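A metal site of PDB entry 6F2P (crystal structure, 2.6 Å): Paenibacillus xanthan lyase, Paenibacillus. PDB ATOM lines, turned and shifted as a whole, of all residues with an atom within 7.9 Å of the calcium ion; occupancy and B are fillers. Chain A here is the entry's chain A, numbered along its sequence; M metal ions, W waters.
The side-chain amide nitrogen (NE2) of Gln 161 sits at hydrogen-bond distance from the backbone carbonyl oxygen (O) of Gln 127 (2.8 Å). O of Gln 161 is in hydrogen-bond range of NH1 of Arg 190 (2.9 Å). The side-chain carboxylate of Glu 174 sits at hydrogen-bond distance from the backbone NH of Thr 165 (3.2 Å). OE1 of Glu 174 lies within hydrogen-bond range of N of Met 166, at 2.9 Å.
Within 4 Å of the calcium ion: Gln 161, Ser 163 and Glu 174. Along chain A the residues within 4 Å of the calcium ion span positions 161 to 174.
The calcium ion is bound by OE1 of Gln 161 (2.2 Å), water W4 (2.3 Å), O of Ser 163 (2.4 Å), water W1 (2.5 Å), water W3 (2.5 Å), OE2 of Glu 174 (2.5 Å) and water W2 (2.6 Å).
Water W1 bridges NE2 of Gln 127 (2.5 Å) and O of Thr 160 (3.2 Å). Water W2 lies within hydrogen-bond range of NE2 of Gln 127 (2.7 Å), NE2 of Gln 161 (3.1 Å) and SD of Met 166 (3.2 Å).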
ATOM      1  N   TRP A 123     -13.768 -16.898  14.530  1.00  0.00           N
ATOM      2  CA  TRP A 123     -13.301 -16.754  13.144  1.00  0.00           C
ATOM      3  C   TRP A 123     -12.302 -15.616  12.971  1.00  0.00           C
ATOM      4  O   TRP A 123     -11.372 -15.694  12.170  1.00  0.00           O
ATOM      5  CB  TRP A 123     -14.499 -16.500  12.233  1.00  0.00           C
ATOM      6  CG  TRP A 123     -15.098 -15.122  12.415  1.00  0.00           C
ATOM      7  CD1 TRP A 123     -16.044 -14.760  13.335  1.00  0.00           C
ATOM      8  CD2 TRP A 123     -14.774 -13.931  11.686  1.00  0.00           C
ATOM      9  NE1 TRP A 123     -16.338 -13.420  13.213  1.00  0.00           N
ATOM     10  CE2 TRP A 123     -15.566 -12.887  12.206  1.00  0.00           C
ATOM     11  CE3 TRP A 123     -13.898 -13.649  10.635  1.00  0.00           C
ATOM     12  CZ2 TRP A 123     -15.499 -11.587  11.715  1.00  0.00           C
ATOM     13  CZ3 TRP A 123     -13.826 -12.357  10.149  1.00  0.00           C
ATOM     14  CH2 TRP A 123     -14.636 -11.339  10.687  1.00  0.00           C
ATOM     15  N   GLN A 127      -8.932 -15.242  10.329  1.00  0.00           N
ATOM     16  CA  GLN A 127      -9.062 -14.534   9.061  1.00  0.00           C
ATOM     17  C   GLN A 127      -8.481 -13.123   9.063  1.00  0.00           C
ATOM     18  O   GLN A 127      -8.197 -12.562   8.000  1.00  0.00           O
ATOM     19  CB  GLN A 127     -10.521 -14.515   8.618  1.00  0.00           C
ATOM     20  CG  GLN A 127     -11.167 -15.898   8.600  1.00  0.00           C
ATOM     21  CD  GLN A 127     -12.553 -15.892   8.012  1.00  0.00           C
ATOM     22  OE1 GLN A 127     -13.365 -16.750   8.326  1.00  0.00           O
ATOM     23  NE2 GLN A 127     -12.844 -14.913   7.157  1.00  0.00           N
ATOM     24  N   ILE A 128      -8.282 -12.546  10.239  1.00  0.00           N
ATOM     25  CA  ILE A 128      -7.842 -11.168  10.313  1.00  0.00           C
ATOM     26  C   ILE A 128      -6.683 -10.948  11.286  1.00  0.00           C
ATOM     27  O   ILE A 128      -5.611 -10.524  10.875  1.00  0.00           O
ATOM     28  CB  ILE A 128      -9.017 -10.236  10.672  1.00  0.00           C
ATOM     29  CG1 ILE A 128     -10.049 -10.231   9.541  1.00  0.00           C
ATOM     30  CG2 ILE A 128      -8.509  -8.838  10.977  1.00  0.00           C
ATOM     31  CD1 ILE A 128     -11.304  -9.478   9.837  1.00  0.00           C
ATOM     32  N   TYR A 159      -5.538 -19.160   2.606  1.00  0.00           N
ATOM     33  CA  TYR A 159      -6.489 -20.166   3.043  1.00  0.00           C
ATOM     34  C   TYR A 159      -7.556 -19.568   3.954  1.00  0.00           C
ATOM     35  O   TYR A 159      -8.754 -19.716   3.688  1.00  0.00           O
ATOM     36  CB  TYR A 159      -5.763 -21.313   3.726  1.00  0.00           C
ATOM     37  CG  TYR A 159      -6.670 -22.236   4.506  1.00  0.00           C
ATOM     38  CD1 TYR A 159      -7.602 -23.037   3.852  1.00  0.00           C
ATOM     39  CD2 TYR A 159      -6.595 -22.307   5.882  1.00  0.00           C
ATOM     40  CE1 TYR A 159      -8.434 -23.876   4.557  1.00  0.00           C
ATOM     41  CE2 TYR A 159      -7.419 -23.158   6.605  1.00  0.00           C
ATOM     42  CZ  TYR A 159      -8.342 -23.937   5.933  1.00  0.00           C
ATOM     43  OH  TYR A 159      -9.171 -24.780   6.651  1.00  0.00           O
ATOM     44  N   THR A 160      -7.130 -18.890   5.014  1.00  0.00           N
ATOM     45  CA  THR A 160      -8.081 -18.290   5.938  1.00  0.00           C
ATOM     46  C   THR A 160      -8.735 -17.020   5.408  1.00  0.00           C
ATOM     47  O   THR A 160      -9.878 -16.718   5.739  1.00  0.00           O
ATOM     48  CB  THR A 160      -7.435 -17.991   7.306  1.00  0.00           C
ATOM     49  OG1 THR A 160      -6.451 -16.962   7.144  1.00  0.00           O
ATOM     50  CG2 THR A 160      -6.798 -19.230   7.885  1.00  0.00           C
ATOM     51  N   GLN A 161      -8.018 -16.271   4.561  1.00  0.00           N
ATOM     52  CA  GLN A 161      -8.536 -14.992   4.058  1.00  0.00           C
ATOM     53  C   GLN A 161      -8.455 -14.915   2.546  1.00  0.00           C
ATOM     54  O   GLN A 161      -7.539 -14.302   1.994  1.00  0.00           O
ATOM     55  CB  GLN A 161      -7.775 -13.835   4.693  1.00  0.00           C
ATOM     56  CG  GLN A 161      -8.339 -12.449   4.378  1.00  0.00           C
ATOM     57  CD  GLN A 161      -9.789 -12.354   4.730  1.00  0.00           C
ATOM     58  OE1 GLN A 161     -10.649 -12.440   3.867  1.00  0.00           O
ATOM     59  NE2 GLN A 161     -10.083 -12.210   6.017  1.00  0.00           N
ATOM     60  N   ALA A 162      -9.432 -15.528   1.878  1.00  0.00           N
ATOM     61  CA  ALA A 162      -9.361 -15.740   0.424  1.00  0.00           C
ATOM     62  C   ALA A 162      -9.882 -14.592  -0.412  1.00  0.00           C
ATOM     63  O   ALA A 162      -9.347 -14.309  -1.476  1.00  0.00           O
ATOM     64  CB  ALA A 162     -10.070 -17.024   0.035  1.00  0.00           C
ATOM     65  N   SER A 163     -10.940 -13.940   0.063  1.00  0.00           N
ATOM     66  CA  SER A 163     -11.577 -12.869  -0.711  1.00  0.00           C
ATOM     67  C   SER A 163     -12.242 -11.854   0.208  1.00  0.00           C
ATOM     68  O   SER A 163     -12.404 -12.105   1.398  1.00  0.00           O
ATOM     69  CB  SER A 163     -12.629 -13.453  -1.632  1.00  0.00           C
ATOM     70  OG  SER A 163     -13.694 -14.001  -0.876  1.00  0.00           O
ATOM     71  N   VAL A 164     -12.633 -10.728  -0.355  1.00  0.00           N
ATOM     72  CA  VAL A 164     -13.367  -9.707   0.378  1.00  0.00           C
ATOM     73  C   VAL A 164     -14.866  -9.949   0.231  1.00  0.00           C
ATOM     74  O   VAL A 164     -15.378  -9.931  -0.877  1.00  0.00           O
ATOM     75  CB  VAL A 164     -13.081  -8.330  -0.197  1.00  0.00           C
ATOM     76  CG1 VAL A 164     -13.905  -7.276   0.534  1.00  0.00           C
ATOM     77  CG2 VAL A 164     -11.598  -8.009  -0.122  1.00  0.00           C
ATOM     78  N   THR A 165     -15.556 -10.186   1.338  1.00  0.00           N
ATOM     79  CA  THR A 165     -17.001 -10.417   1.265  1.00  0.00           C
ATOM     80  C   THR A 165     -17.790  -9.667   2.340  1.00  0.00           C
ATOM     81  O   THR A 165     -19.016  -9.544   2.273  1.00  0.00           O
ATOM     82  CB  THR A 165     -17.376 -11.908   1.401  1.00  0.00           C
ATOM     83  OG1 THR A 165     -17.269 -12.300   2.782  1.00  0.00           O
ATOM     84  CG2 THR A 165     -16.490 -12.783   0.527  1.00  0.00           C
ATOM     85  N   MET A 166     -17.080  -9.171   3.344  1.00  0.00           N
ATOM     86  CA  MET A 166     -17.733  -8.637   4.534  1.00  0.00           C
ATOM     87  C   MET A 166     -18.011  -7.150   4.418  1.00  0.00           C
ATOM     88  O   MET A 166     -17.839  -6.559   3.349  1.00  0.00           O
ATOM     89  CB  MET A 166     -16.892  -8.957   5.761  1.00  0.00           C
ATOM     90  CG  MET A 166     -16.565 -10.429   5.848  1.00  0.00           C
ATOM     91  SD  MET A 166     -15.629 -10.871   7.306  1.00  0.00           S
ATOM     92  CE  MET A 166     -16.187 -12.558   7.508  1.00  0.00           C
ATOM     93  N   ASN A 170     -14.578  -5.060   9.061  1.00  0.00           N
ATOM     94  CA  ASN A 170     -14.118  -6.380   8.654  1.00  0.00           C
ATOM     95  C   ASN A 170     -13.687  -6.373   7.209  1.00  0.00           C
ATOM     96  O   ASN A 170     -12.710  -7.022   6.825  1.00  0.00           O
ATOM     97  CB  ASN A 170     -15.218  -7.428   8.842  1.00  0.00           C
ATOM     98  CG  ASN A 170     -15.527  -7.691  10.283  1.00  0.00           C
ATOM     99  OD1 ASN A 170     -14.678  -7.508  11.167  1.00  0.00           O
ATOM    100  ND2 ASN A 170     -16.750  -8.129  10.541  1.00  0.00           N
ATOM    101  N   ARG A 171     -14.438  -5.617   6.402  1.00  0.00           N
ATOM    102  CA  ARG A 171     -14.166  -5.559   4.988  1.00  0.00           C
ATOM    103  C   ARG A 171     -12.842  -4.862   4.749  1.00  0.00           C
ATOM    104  O   ARG A 171     -12.054  -5.268   3.903  1.00  0.00           O
ATOM    105  CB  ARG A 171     -15.267  -4.818   4.264  1.00  0.00           C
ATOM    106  CG  ARG A 171     -15.034  -4.701   2.770  1.00  0.00           C
ATOM    107  CD  ARG A 171     -16.232  -4.108   2.056  1.00  0.00           C
ATOM    108  NE  ARG A 171     -16.053  -4.227   0.620  1.00  0.00           N
ATOM    109  CZ  ARG A 171     -16.541  -5.223  -0.102  1.00  0.00           C
ATOM    110  NH1 ARG A 171     -16.301  -5.259  -1.416  1.00  0.00           N
ATOM    111  NH2 ARG A 171     -17.274  -6.175   0.462  1.00  0.00           N
ATOM    112  N   TRP A 173     -10.326  -4.737   6.889  1.00  0.00           N
ATOM    113  CA  TRP A 173      -9.284  -5.649   7.340  1.00  0.00           C
ATOM    114  C   TRP A 173      -9.073  -6.789   6.361  1.00  0.00           C
ATOM    115  O   TRP A 173      -7.936  -7.226   6.166  1.00  0.00           O
ATOM    116  CB  TRP A 173      -9.616  -6.188   8.718  1.00  0.00           C
ATOM    117  CG  TRP A 173      -9.657  -5.113   9.720  1.00  0.00           C
ATOM    118  CD1 TRP A 173      -8.913  -3.968   9.721  1.00  0.00           C
ATOM    119  CD2 TRP A 173     -10.513  -5.037  10.864  1.00  0.00           C
ATOM    120  NE1 TRP A 173      -9.246  -3.197  10.812  1.00  0.00           N
ATOM    121  CE2 TRP A 173     -10.225  -3.833  11.527  1.00  0.00           C
ATOM    122  CE3 TRP A 173     -11.496  -5.890  11.394  1.00  0.00           C
ATOM    123  CZ2 TRP A 173     -10.879  -3.452  12.705  1.00  0.00           C
ATOM    124  CZ3 TRP A 173     -12.153  -5.505  12.559  1.00  0.00           C
ATOM    125  CH2 TRP A 173     -11.835  -4.293  13.203  1.00  0.00           C
ATOM    126  N   GLU A 174     -10.159  -7.275   5.779  1.00  0.00           N
ATOM    127  CA  GLU A 174     -10.048  -8.239   4.689  1.00  0.00           C
ATOM    128  C   GLU A 174      -9.111  -7.653   3.640  1.00  0.00           C
ATOM    129  O   GLU A 174      -8.166  -8.311   3.186  1.00  0.00           O
ATOM    130  CB  GLU A 174     -11.415  -8.498   4.054  1.00  0.00           C
ATOM    131  CG  GLU A 174     -12.295  -9.488   4.780  1.00  0.00           C
ATOM    132  CD  GLU A 174     -13.639  -9.654   4.099  1.00  0.00           C
ATOM    133  OE1 GLU A 174     -14.320  -8.649   3.847  1.00  0.00           O
ATOM    134  OE2 GLU A 174     -14.022 -10.813   3.797  1.00  0.00           O
ATOM    135  N   SER A 175      -9.377  -6.394   3.281  1.00  0.00           N
ATOM    136  CA  SER A 175      -8.678  -5.728   2.199  1.00  0.00           C
ATOM    137  C   SER A 175      -7.220  -5.522   2.531  1.00  0.00           C
ATOM    138  O   SER A 175      -6.371  -5.797   1.685  1.00  0.00           O
ATOM    139  CB  SER A 175      -9.342  -4.392   1.838  1.00  0.00           C
ATOM    140  OG  SER A 175     -10.718  -4.574   1.570  1.00  0.00           O
ATOM    141  N   ILE A 178      -5.494  -8.969   2.535  1.00  0.00           N
ATOM    142  CA  ILE A 178      -5.376  -9.445   1.165  1.00  0.00           C
ATOM    143  C   ILE A 178      -4.328  -8.657   0.387  1.00  0.00           C
ATOM    144  O   ILE A 178      -3.496  -9.241  -0.315  1.00  0.00           O
ATOM    145  CB  ILE A 178      -6.733  -9.436   0.459  1.00  0.00           C
ATOM    146  CG1 ILE A 178      -7.542 -10.633   0.958  1.00  0.00           C
ATOM    147  CG2 ILE A 178      -6.567  -9.480  -1.035  1.00  0.00           C
ATOM    148  CD1 ILE A 178      -8.968 -10.630   0.519  1.00  0.00           C
ATOM    149  N   ARG A 190      -3.877 -10.555  -6.477  1.00  0.00           N
ATOM    150  CA  ARG A 190      -4.240 -10.541  -5.070  1.00  0.00           C
ATOM    151  C   ARG A 190      -4.171  -9.119  -4.520  1.00  0.00           C
ATOM    152  O   ARG A 190      -5.049  -8.705  -3.765  1.00  0.00           O
ATOM    153  CB  ARG A 190      -3.335 -11.513  -4.279  1.00  0.00           C
ATOM    154  CG  ARG A 190      -3.490 -11.488  -2.784  1.00  0.00           C
ATOM    155  CD  ARG A 190      -4.371 -12.603  -2.249  1.00  0.00           C
ATOM    156  NE  ARG A 190      -4.214 -12.729  -0.807  1.00  0.00           N
ATOM    157  CZ  ARG A 190      -5.081 -13.350  -0.006  1.00  0.00           C
ATOM    158  NH1 ARG A 190      -6.184 -13.899  -0.497  1.00  0.00           N
ATOM    159  NH2 ARG A 190      -4.832 -13.404   1.303  1.00  0.00           N
HETATM  160 CA    CA M   1     -12.811 -12.970   3.562  1.00  0.00          CA
HETATM  161  O   HOH W   1     -12.453 -15.119   4.691  1.00  0.00           O
HETATM  162  O   HOH W   2     -13.195 -12.524   6.046  1.00  0.00           O
HETATM  163  O   HOH W   3     -13.121 -14.743   1.883  1.00  0.00           O
HETATM  164  O   HOH W   4     -14.929 -13.859   3.859  1.00  0.00           O
